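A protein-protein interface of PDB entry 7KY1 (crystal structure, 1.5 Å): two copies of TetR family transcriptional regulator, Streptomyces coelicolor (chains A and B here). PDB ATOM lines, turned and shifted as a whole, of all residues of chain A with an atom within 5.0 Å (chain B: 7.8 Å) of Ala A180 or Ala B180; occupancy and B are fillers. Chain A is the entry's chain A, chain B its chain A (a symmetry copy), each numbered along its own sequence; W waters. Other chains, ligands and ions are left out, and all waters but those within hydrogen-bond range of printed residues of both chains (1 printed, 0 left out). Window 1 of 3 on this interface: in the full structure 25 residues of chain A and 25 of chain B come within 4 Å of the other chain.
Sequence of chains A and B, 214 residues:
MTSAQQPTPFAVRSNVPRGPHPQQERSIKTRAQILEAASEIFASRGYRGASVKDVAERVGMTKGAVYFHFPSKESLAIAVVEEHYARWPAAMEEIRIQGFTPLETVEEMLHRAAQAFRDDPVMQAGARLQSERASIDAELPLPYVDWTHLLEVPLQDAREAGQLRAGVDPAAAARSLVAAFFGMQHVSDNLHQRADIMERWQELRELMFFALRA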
ATOM      1  N   ARG A 175      -1.849  -3.261 -14.478  1.00  0.00           N
ATOM      2  CA  ARG A 175      -1.904  -1.987 -13.771  1.00  0.00           C
ATOM      3  C   ARG A 175      -1.898  -2.200 -12.274  1.00  0.00           C
ATOM      4  O   ARG A 175      -1.174  -1.502 -11.552  1.00  0.00           O
ATOM      5  CB  ARG A 175      -3.149  -1.180 -14.179  1.00  0.00           C
ATOM      6  CG  ARG A 175      -3.112  -0.670 -15.627  1.00  0.00           C
ATOM      7  CD  ARG A 175      -4.297   0.227 -15.956  1.00  0.00           C
ATOM      8  NE  ARG A 175      -5.583  -0.481 -15.952  1.00  0.00           N
ATOM      9  CZ  ARG A 175      -6.161  -1.004 -17.031  1.00  0.00           C
ATOM     10  NH1 ARG A 175      -5.572  -0.917 -18.217  1.00  0.00           N
ATOM     11  NH2 ARG A 175      -7.334  -1.619 -16.914  1.00  0.00           N
ATOM     12  N   SER A 176      -2.685  -3.176 -11.791  1.00  0.00           N
ATOM     13  CA  SER A 176      -2.819  -3.377 -10.351  1.00  0.00           C
ATOM     14  C   SER A 176      -1.518  -3.879  -9.754  1.00  0.00           C
ATOM     15  O   SER A 176      -1.095  -3.414  -8.690  1.00  0.00           O
ATOM     16  CB  SER A 176      -3.952  -4.359 -10.048  1.00  0.00           C
ATOM     17  OG  SER A 176      -5.190  -3.829 -10.508  1.00  0.00           O
ATOM     18  N   LEU A 177      -0.847  -4.795 -10.453  1.00  0.00           N
ATOM     19  CA  LEU A 177       0.419  -5.309  -9.949  1.00  0.00           C
ATOM     20  C   LEU A 177       1.483  -4.221  -9.901  1.00  0.00           C
ATOM     21  O   LEU A 177       2.245  -4.134  -8.932  1.00  0.00           O
ATOM     22  CB  LEU A 177       0.901  -6.471 -10.825  1.00  0.00           C
ATOM     23  CG  LEU A 177       0.212  -7.813 -10.605  1.00  0.00           C
ATOM     24  CD1 LEU A 177       0.537  -8.728 -11.759  1.00  0.00           C
ATOM     25  CD2 LEU A 177       0.706  -8.437  -9.309  1.00  0.00           C
ATOM     26  N   VAL A 178       1.607  -3.430 -10.968  1.00  0.00           N
ATOM     27  CA  VAL A 178       2.634  -2.389 -10.992  1.00  0.00           C
ATOM     28  C   VAL A 178       2.382  -1.373  -9.885  1.00  0.00           C
ATOM     29  O   VAL A 178       3.306  -0.961  -9.176  1.00  0.00           O
ATOM     30  CB  VAL A 178       2.686  -1.729 -12.386  1.00  0.00           C
ATOM     31  CG1 VAL A 178       3.508  -0.450 -12.347  1.00  0.00           C
ATOM     32  CG2 VAL A 178       3.289  -2.687 -13.390  1.00  0.00           C
ATOM     33  N   ALA A 179       1.123  -0.966  -9.703  1.00  0.00           N
ATOM     34  CA  ALA A 179       0.791   0.001  -8.663  1.00  0.00           C
ATOM     35  C   ALA A 179       1.066  -0.564  -7.279  1.00  0.00           C
ATOM     36  O   ALA A 179       1.649   0.112  -6.415  1.00  0.00           O
ATOM     37  CB  ALA A 179      -0.677   0.410  -8.780  1.00  0.00           C
ATOM     38  N   ALA A 180       0.633  -1.797  -7.037  1.00  0.00           N
ATOM     39  CA  ALA A 180       0.793  -2.376  -5.707  1.00  0.00           C
ATOM     40  C   ALA A 180       2.258  -2.635  -5.390  1.00  0.00           C
ATOM     41  O   ALA A 180       2.723  -2.379  -4.265  1.00  0.00           O
ATOM     42  CB  ALA A 180      -0.009  -3.661  -5.602  1.00  0.00           C
ATOM     43  N   PHE A 181       3.001  -3.141  -6.372  1.00  0.00           N
ATOM     44  CA  PHE A 181       4.418  -3.362  -6.159  1.00  0.00           C
ATOM     45  C   PHE A 181       5.128  -2.053  -5.874  1.00  0.00           C
ATOM     46  O   PHE A 181       5.925  -1.962  -4.940  1.00  0.00           O
ATOM     47  CB  PHE A 181       5.052  -4.048  -7.365  1.00  0.00           C
ATOM     48  CG  PHE A 181       6.485  -4.403  -7.133  1.00  0.00           C
ATOM     49  CD1 PHE A 181       7.495  -3.493  -7.399  1.00  0.00           C
ATOM     50  CD2 PHE A 181       6.806  -5.633  -6.600  1.00  0.00           C
ATOM     51  CE1 PHE A 181       8.823  -3.831  -7.154  1.00  0.00           C
ATOM     52  CE2 PHE A 181       8.108  -5.968  -6.364  1.00  0.00           C
ATOM     53  CZ  PHE A 181       9.115  -5.070  -6.635  1.00  0.00           C
ATOM     54  N   PHE A 182       4.861  -1.022  -6.679  1.00  0.00           N
ATOM     55  CA  PHE A 182       5.494   0.263  -6.428  1.00  0.00           C
ATOM     56  C   PHE A 182       5.202   0.743  -5.010  1.00  0.00           C
ATOM     57  O   PHE A 182       6.085   1.264  -4.301  1.00  0.00           O
ATOM     58  CB  PHE A 182       5.013   1.321  -7.432  1.00  0.00           C
ATOM     59  CG  PHE A 182       5.286   2.714  -6.942  1.00  0.00           C
ATOM     60  CD1 PHE A 182       6.560   3.259  -7.047  1.00  0.00           C
ATOM     61  CD2 PHE A 182       4.306   3.432  -6.266  1.00  0.00           C
ATOM     62  CE1 PHE A 182       6.835   4.517  -6.527  1.00  0.00           C
ATOM     63  CE2 PHE A 182       4.569   4.688  -5.750  1.00  0.00           C
ATOM     64  CZ  PHE A 182       5.840   5.230  -5.876  1.00  0.00           C
ATOM     65  N   GLY A 183       3.944   0.621  -4.593  1.00  0.00           N
ATOM     66  CA  GLY A 183       3.577   1.100  -3.270  1.00  0.00           C
ATOM     67  C   GLY A 183       4.323   0.359  -2.179  1.00  0.00           C
ATOM     68  O   GLY A 183       4.868   0.962  -1.254  1.00  0.00           O
ATOM     69  N   MET A 184       4.366  -0.967  -2.298  1.00  0.00           N
ATOM     70  CA  MET A 184       5.073  -1.799  -1.335  1.00  0.00           C
ATOM     71  C   MET A 184       6.527  -1.372  -1.204  1.00  0.00           C
ATOM     72  O   MET A 184       7.018  -1.155  -0.094  1.00  0.00           O
ATOM     73  CB  MET A 184       4.949  -3.261  -1.780  1.00  0.00           C
ATOM     74  CG  MET A 184       5.642  -4.317  -0.923  1.00  0.00           C
ATOM     75  SD  MET A 184       7.417  -4.463  -1.256  1.00  0.00           S
ATOM     76  CE  MET A 184       7.540  -4.737  -3.026  1.00  0.00           C
ATOM     77  N   LEU A 204       2.476  -9.526   0.042  1.00  0.00           N
ATOM     78  CA  LEU A 204       1.632  -8.925  -0.991  1.00  0.00           C
ATOM     79  C   LEU A 204       1.486  -9.856  -2.184  1.00  0.00           C
ATOM     80  O   LEU A 204       0.373 -10.058  -2.687  1.00  0.00           O
ATOM     81  CB  LEU A 204       2.223  -7.584  -1.430  1.00  0.00           C
ATOM     82  CG  LEU A 204       1.512  -6.872  -2.579  1.00  0.00           C
ATOM     83  CD1 LEU A 204       0.088  -6.557  -2.190  1.00  0.00           C
ATOM     84  CD2 LEU A 204       2.271  -5.586  -2.926  1.00  0.00           C
ATOM     85  N   MET A 208      -1.932 -11.174  -4.078  1.00  0.00           N
ATOM     86  CA  MET A 208      -2.249 -10.818  -5.448  1.00  0.00           C
ATOM     87  C   MET A 208      -2.248 -12.048  -6.353  1.00  0.00           C
ATOM     88  O   MET A 208      -3.155 -12.203  -7.175  1.00  0.00           O
ATOM     89  CB  MET A 208      -1.290  -9.733  -5.933  1.00  0.00           C
ATOM     90  CG  MET A 208      -1.349  -8.483  -5.038  1.00  0.00           C
ATOM     91  SD  MET A 208      -0.752  -6.975  -5.820  1.00  0.00           S
ATOM     92  CE  MET A 208      -2.039  -6.641  -7.043  1.00  0.00           C
ATOM     93  N   LEU B 110     -11.469   2.197   2.427  1.00  0.00           N
ATOM     94  CA  LEU B 110     -10.607   2.500   1.297  1.00  0.00           C
ATOM     95  C   LEU B 110     -11.375   3.153   0.153  1.00  0.00           C
ATOM     96  O   LEU B 110     -10.815   4.004  -0.545  1.00  0.00           O
ATOM     97  CB  LEU B 110      -9.901   1.227   0.834  1.00  0.00           C
ATOM     98  CG  LEU B 110      -8.939   0.730   1.911  1.00  0.00           C
ATOM     99  CD1 LEU B 110      -8.451  -0.648   1.528  1.00  0.00           C
ATOM    100  CD2 LEU B 110      -7.773   1.680   2.054  1.00  0.00           C
ATOM    101  N   ALA B 173      -2.290  -8.434   5.974  1.00  0.00           N
ATOM    102  CA  ALA B 173      -3.303  -7.881   5.080  1.00  0.00           C
ATOM    103  C   ALA B 173      -3.358  -6.364   5.194  1.00  0.00           C
ATOM    104  O   ALA B 173      -3.534  -5.673   4.181  1.00  0.00           O
ATOM    105  CB  ALA B 173      -4.657  -8.503   5.394  1.00  0.00           C
ATOM    106  N   ALA B 174      -3.225  -5.828   6.422  1.00  0.00           N
ATOM    107  CA  ALA B 174      -3.284  -4.380   6.607  1.00  0.00           C
ATOM    108  C   ALA B 174      -2.121  -3.715   5.904  1.00  0.00           C
ATOM    109  O   ALA B 174      -2.304  -2.747   5.147  1.00  0.00           O
ATOM    110  CB  ALA B 174      -3.295  -4.028   8.096  1.00  0.00           C
ATOM    111  N   ARG B 175      -0.919  -4.259   6.098  1.00  0.00           N
ATOM    112  CA  ARG B 175       0.251  -3.700   5.429  1.00  0.00           C
ATOM    113  C   ARG B 175       0.087  -3.747   3.927  1.00  0.00           C
ATOM    114  O   ARG B 175       0.386  -2.762   3.240  1.00  0.00           O
ATOM    115  CB  ARG B 175       1.532  -4.447   5.838  1.00  0.00           C
ATOM    116  CG  ARG B 175       1.941  -4.225   7.302  1.00  0.00           C
ATOM    117  CD  ARG B 175       3.276  -4.875   7.636  1.00  0.00           C
ATOM    118  NE  ARG B 175       3.239  -6.342   7.586  1.00  0.00           N
ATOM    119  CZ  ARG B 175       3.020  -7.128   8.638  1.00  0.00           C
ATOM    120  NH1 ARG B 175       2.805  -6.602   9.837  1.00  0.00           N
ATOM    121  NH2 ARG B 175       3.016  -8.448   8.481  1.00  0.00           N
ATOM    122  N   SER B 176      -0.409  -4.879   3.400  1.00  0.00           N
ATOM    123  CA  SER B 176      -0.499  -5.047   1.951  1.00  0.00           C
ATOM    124  C   SER B 176      -1.532  -4.103   1.364  1.00  0.00           C
ATOM    125  O   SER B 176      -1.294  -3.482   0.323  1.00  0.00           O
ATOM    126  CB  SER B 176      -0.844  -6.494   1.598  1.00  0.00           C
ATOM    127  OG  SER B 176       0.187  -7.364   2.051  1.00  0.00           O
ATOM    128  N   LEU B 177      -2.666  -3.950   2.047  1.00  0.00           N
ATOM    129  CA  LEU B 177      -3.696  -3.046   1.552  1.00  0.00           C
ATOM    130  C   LEU B 177      -3.218  -1.601   1.556  1.00  0.00           C
ATOM    131  O   LEU B 177      -3.473  -0.855   0.604  1.00  0.00           O
ATOM    132  CB  LEU B 177      -4.966  -3.179   2.400  1.00  0.00           C
ATOM    133  CG  LEU B 177      -5.836  -4.400   2.127  1.00  0.00           C
ATOM    134  CD1 LEU B 177      -6.819  -4.566   3.258  1.00  0.00           C
ATOM    135  CD2 LEU B 177      -6.592  -4.208   0.822  1.00  0.00           C
ATOM    136  N   VAL B 178      -2.593  -1.160   2.649  1.00  0.00           N
ATOM    137  CA  VAL B 178      -2.141   0.229   2.724  1.00  0.00           C
ATOM    138  C   VAL B 178      -1.103   0.505   1.644  1.00  0.00           C
ATOM    139  O   VAL B 178      -1.148   1.537   0.966  1.00  0.00           O
ATOM    140  CB  VAL B 178      -1.605   0.536   4.138  1.00  0.00           C
ATOM    141  CG1 VAL B 178      -0.846   1.854   4.153  1.00  0.00           C
ATOM    142  CG2 VAL B 178      -2.751   0.601   5.124  1.00  0.00           C
ATOM    143  N   ALA B 179      -0.159  -0.420   1.451  1.00  0.00           N
ATOM    144  CA  ALA B 179       0.871  -0.238   0.435  1.00  0.00           C
ATOM    145  C   ALA B 179       0.269  -0.211  -0.960  1.00  0.00           C
ATOM    146  O   ALA B 179       0.618   0.643  -1.791  1.00  0.00           O
ATOM    147  CB  ALA B 179       1.907  -1.358   0.537  1.00  0.00           C
ATOM    148  N   ALA B 180      -0.622  -1.155  -1.247  1.00  0.00           N
ATOM    149  CA  ALA B 180      -1.185  -1.238  -2.592  1.00  0.00           C
ATOM    150  C   ALA B 180      -2.083  -0.047  -2.889  1.00  0.00           C
ATOM    151  O   ALA B 180      -2.047   0.518  -3.996  1.00  0.00           O
ATOM    152  CB  ALA B 180      -1.955  -2.537  -2.751  1.00  0.00           C
ATOM    153  N   PHE B 181      -2.891   0.351  -1.909  1.00  0.00           N
ATOM    154  CA  PHE B 181      -3.736   1.514  -2.102  1.00  0.00           C
ATOM    155  C   PHE B 181      -2.894   2.754  -2.334  1.00  0.00           C
ATOM    156  O   PHE B 181      -3.163   3.532  -3.250  1.00  0.00           O
ATOM    157  CB  PHE B 181      -4.658   1.725  -0.906  1.00  0.00           C
ATOM    158  CG  PHE B 181      -5.628   2.842  -1.122  1.00  0.00           C
ATOM    159  CD1 PHE B 181      -5.289   4.147  -0.810  1.00  0.00           C
ATOM    160  CD2 PHE B 181      -6.858   2.578  -1.687  1.00  0.00           C
ATOM    161  CE1 PHE B 181      -6.196   5.179  -1.041  1.00  0.00           C
ATOM    162  CE2 PHE B 181      -7.749   3.587  -1.909  1.00  0.00           C
ATOM    163  CZ  PHE B 181      -7.420   4.885  -1.592  1.00  0.00           C
ATOM    164  N   PHE B 182      -1.871   2.966  -1.503  1.00  0.00           N
ATOM    165  CA  PHE B 182      -1.017   4.126  -1.703  1.00  0.00           C
ATOM    166  C   PHE B 182      -0.430   4.129  -3.111  1.00  0.00           C
ATOM    167  O   PHE B 182      -0.361   5.175  -3.787  1.00  0.00           O
ATOM    168  CB  PHE B 182       0.125   4.154  -0.676  1.00  0.00           C
ATOM    169  CG  PHE B 182       1.245   5.050  -1.118  1.00  0.00           C
ATOM    170  CD1 PHE B 182       1.142   6.429  -0.972  1.00  0.00           C
ATOM    171  CD2 PHE B 182       2.346   4.531  -1.790  1.00  0.00           C
ATOM    172  CE1 PHE B 182       2.141   7.267  -1.448  1.00  0.00           C
ATOM    173  CE2 PHE B 182       3.350   5.357  -2.263  1.00  0.00           C
ATOM    174  CZ  PHE B 182       3.244   6.730  -2.096  1.00  0.00           C
ATOM    175  N   GLY B 183       0.048   2.970  -3.555  1.00  0.00           N
ATOM    176  CA  GLY B 183       0.666   2.904  -4.869  1.00  0.00           C
ATOM    177  C   GLY B 183      -0.314   3.260  -5.968  1.00  0.00           C
ATOM    178  O   GLY B 183      -0.013   4.049  -6.864  1.00  0.00           O
ATOM    179  N   MET B 184      -1.513   2.685  -5.889  1.00  0.00           N
ATOM    180  CA  MET B 184      -2.559   2.961  -6.864  1.00  0.00           C
ATOM    181  C   MET B 184      -2.846   4.452  -6.954  1.00  0.00           C
ATOM    182  O   MET B 184      -2.859   5.021  -8.048  1.00  0.00           O
ATOM    183  CB  MET B 184      -3.808   2.166  -6.466  1.00  0.00           C
ATOM    184  CG  MET B 184      -5.049   2.322  -7.341  1.00  0.00           C
ATOM    185  SD  MET B 184      -6.000   3.821  -6.980  1.00  0.00           S
ATOM    186  CE  MET B 184      -6.333   3.750  -5.217  1.00  0.00           C
ATOM    187  N   GLN B 185      -3.079   5.108  -5.808  1.00  0.00           N
ATOM    188  CA  GLN B 185      -3.466   6.513  -5.881  1.00  0.00           C
ATOM    189  C   GLN B 185      -2.294   7.361  -6.339  1.00  0.00           C
ATOM    190  O   GLN B 185      -2.483   8.346  -7.063  1.00  0.00           O
ATOM    191  CB  GLN B 185      -4.013   7.004  -4.525  1.00  0.00           C
ATOM    192  CG  GLN B 185      -2.988   7.135  -3.390  1.00  0.00           C
ATOM    193  CD  GLN B 185      -2.156   8.411  -3.470  1.00  0.00           C
ATOM    194  OE1 GLN B 185      -2.538   9.384  -4.126  1.00  0.00           O
ATOM    195  NE2 GLN B 185      -1.012   8.404  -2.810  1.00  0.00           N
ATOM    196  N   HIS B 186      -1.077   6.956  -5.976  1.00  0.00           N
ATOM    197  CA  HIS B 186       0.108   7.707  -6.369  1.00  0.00           C
ATOM    198  C   HIS B 186       0.355   7.617  -7.875  1.00  0.00           C
ATOM    199  O   HIS B 186       0.643   8.628  -8.531  1.00  0.00           O
ATOM    200  CB  HIS B 186       1.314   7.191  -5.591  1.00  0.00           C
ATOM    201  CG  HIS B 186       2.519   8.061  -5.725  1.00  0.00           C
ATOM    202  ND1 HIS B 186       2.693   9.209  -4.980  1.00  0.00           N
ATOM    203  CD2 HIS B 186       3.602   7.961  -6.529  1.00  0.00           C
ATOM    204  CE1 HIS B 186       3.846   9.766  -5.306  1.00  0.00           C
ATOM    205  NE2 HIS B 186       4.413   9.033  -6.247  1.00  0.00           N
ATOM    206  N   VAL B 187       0.250   6.415  -8.442  1.00  0.00           N
ATOM    207  CA  VAL B 187       0.351   6.258  -9.890  1.00  0.00           C
ATOM    208  C   VAL B 187      -0.710   7.099 -10.587  1.00  0.00           C
ATOM    209  O   VAL B 187      -0.438   7.791 -11.574  1.00  0.00           O
ATOM    210  CB  VAL B 187       0.221   4.774 -10.288  1.00  0.00           C
ATOM    211  CG1 VAL B 187       0.109   4.647 -11.792  1.00  0.00           C
ATOM    212  CG2 VAL B 187       1.419   3.958  -9.790  1.00  0.00           C
ATOM    213  N   ARG B 200      -9.146   2.781 -11.235  1.00  0.00           N
ATOM    214  CA  ARG B 200      -7.963   2.038 -10.797  1.00  0.00           C
ATOM    215  C   ARG B 200      -8.191   1.381  -9.447  1.00  0.00           C
ATOM    216  O   ARG B 200      -7.769   0.237  -9.236  1.00  0.00           O
ATOM    217  CB  ARG B 200      -6.750   2.952 -10.726  1.00  0.00           C
ATOM    218  CG  ARG B 200      -6.421   3.688 -12.026  1.00  0.00           C
ATOM    219  CD  ARG B 200      -5.809   2.782 -13.112  1.00  0.00           C
ATOM    220  NE  ARG B 200      -6.777   1.886 -13.733  1.00  0.00           N
ATOM    221  CZ  ARG B 200      -7.650   2.254 -14.671  1.00  0.00           C
ATOM    222  NH1 ARG B 200      -7.705   3.521 -15.097  1.00  0.00           N
ATOM    223  NH2 ARG B 200      -8.491   1.356 -15.169  1.00  0.00           N
ATOM    224  N   TRP B 201      -8.868   2.067  -8.528  1.00  0.00           N
ATOM    225  CA  TRP B 201      -9.142   1.427  -7.247  1.00  0.00           C
ATOM    226  C   TRP B 201     -10.082   0.250  -7.413  1.00  0.00           C
ATOM    227  O   TRP B 201      -9.857  -0.809  -6.818  1.00  0.00           O
ATOM    228  CB  TRP B 201      -9.708   2.409  -6.219  1.00  0.00           C
ATOM    229  CG  TRP B 201     -10.079   1.666  -4.931  1.00  0.00           C
ATOM    230  CD1 TRP B 201     -11.300   1.637  -4.322  1.00  0.00           C
ATOM    231  CD2 TRP B 201      -9.225   0.799  -4.159  1.00  0.00           C
ATOM    232  NE1 TRP B 201     -11.254   0.838  -3.211  1.00  0.00           N
ATOM    233  CE2 TRP B 201      -9.990   0.316  -3.083  1.00  0.00           C
ATOM    234  CE3 TRP B 201      -7.882   0.412  -4.261  1.00  0.00           C
ATOM    235  CZ2 TRP B 201      -9.469  -0.554  -2.128  1.00  0.00           C
ATOM    236  CZ3 TRP B 201      -7.365  -0.459  -3.309  1.00  0.00           C
ATOM    237  CH2 TRP B 201      -8.159  -0.922  -2.253  1.00  0.00           C
ATOM    238  N   LEU B 204      -8.199  -2.851  -8.524  1.00  0.00           N
ATOM    239  CA  LEU B 204      -7.298  -3.356  -7.489  1.00  0.00           C
ATOM    240  C   LEU B 204      -8.078  -3.949  -6.328  1.00  0.00           C
ATOM    241  O   LEU B 204      -7.756  -5.045  -5.852  1.00  0.00           O
ATOM    242  CB  LEU B 204      -6.387  -2.229  -6.998  1.00  0.00           C
ATOM    243  CG  LEU B 204      -5.448  -2.569  -5.842  1.00  0.00           C
ATOM    244  CD1 LEU B 204      -4.507  -3.676  -6.248  1.00  0.00           C
ATOM    245  CD2 LEU B 204      -4.662  -1.314  -5.441  1.00  0.00           C
ATOM    246  N   MET B 208      -7.712  -7.647  -4.539  1.00  0.00           N
ATOM    247  CA  MET B 208      -7.276  -7.808  -3.165  1.00  0.00           C
ATOM    248  C   MET B 208      -8.385  -8.399  -2.298  1.00  0.00           C
ATOM    249  O   MET B 208      -8.121  -9.300  -1.498  1.00  0.00           O
ATOM    250  CB  MET B 208      -6.763  -6.472  -2.629  1.00  0.00           C
ATOM    251  CG  MET B 208      -5.610  -5.923  -3.487  1.00  0.00           C
ATOM    252  SD  MET B 208      -4.560  -4.725  -2.648  1.00  0.00           S
ATOM    253  CE  MET B 208      -3.694  -5.751  -1.440  1.00  0.00           C
HETATM  254  O   HOH W   1      -5.376  -0.673 -10.608  1.00  0.00           O
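NE of Arg A175 lies close to NE of Arg B200, 3.5 Å away.
NE2 of Gln B185 sits close to O of Phe B182 (3.4 Å).
The backbone NH (N) of Trp B201 lies within hydrogen-bond range of the side-chain sulfur (SD) of Met B184 (3.7 Å).
Among the printed residues, pairs that only touch across the chains: Ala A179 with Gly B183, Gly A183 with Ala B179, Phe A182 with His B186, Ala A180 with Ala B180, Ala A179 with Met B184, Met A184 with Ala B179, Leu A204 with Ser B176, Ser A176 with Leu B204, Phe A182 with Phe B182, Gly A183 with Gly B183, Gly A183 with Phe B182, Phe A182 with Gly B183, Met A208 with Leu B204 and Leu A204 with Met B208.
Of the printed residues of chain B, Arg A175 touches Arg B200.
Of the printed residues of chain B, Ala A179 touches Gly B183 (3.3 Å) and Met B184 (3.7 Å).
Ala A180 touches one residue of chain B.
Of the printed residues of chain B, Met A208 touches Leu B204.
Arg B175 touches none of the printed residues of chain A.
Ala B180 touches one residue of chain A.
Printed residues of chain A within 4 Å of Gly B183: Ala A179 (3.3 Å), Phe A182 (3.9 Å) and Gly A183 (3.8 Å).
The nearest residue of chain B that does not touch Ala A180 is Ala B179 (4.4 Å).
The nearest residue of chain A that does not touch Ala B180 is Ala A179 (4.4 Å).
Hydrophobic or aromatic side chains of chain A within 4 Å of the printed part of chain B: Ala A179, Ala A180, Phe A182, Leu A204 and Met A208.
Along chain A the printed residues that touch a printed residue of chain B span positions 175 to 208.
Of the 20 printed residues of chain B, 10 touch a printed residue of chain A.
Hydrophobic or aromatic side chains of chain B that line the printed part of chain A: Ala B179, Ala B180, Phe B182, His B186, Leu B204 and Met B208.
Among the printed residues, 15 pairs touch across the chains.
Ala A179 touches Met B184, and with the chains exchanged Met A184 touches Ala B179.
Phe B182 touches its own counterpart, Phe A182.
Phe A182 touches Gly B183, and with the chains exchanged Gly A183 touches Phe B182.
Leu A204 touches Met B208, and with the chains exchanged Met A208 touches Leu B204.
Positions printed for both chains: 175, 176, 177, 178, 179, 180, 181, 182, 183, 184, 204 and 208.
Of the 15 pairs that touch across the chains among the printed residues, 13 have their exchanged pair printed and touching as well.
Water W1 lies within hydrogen-bond range of O of Arg B200 and OG of Ser A176.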
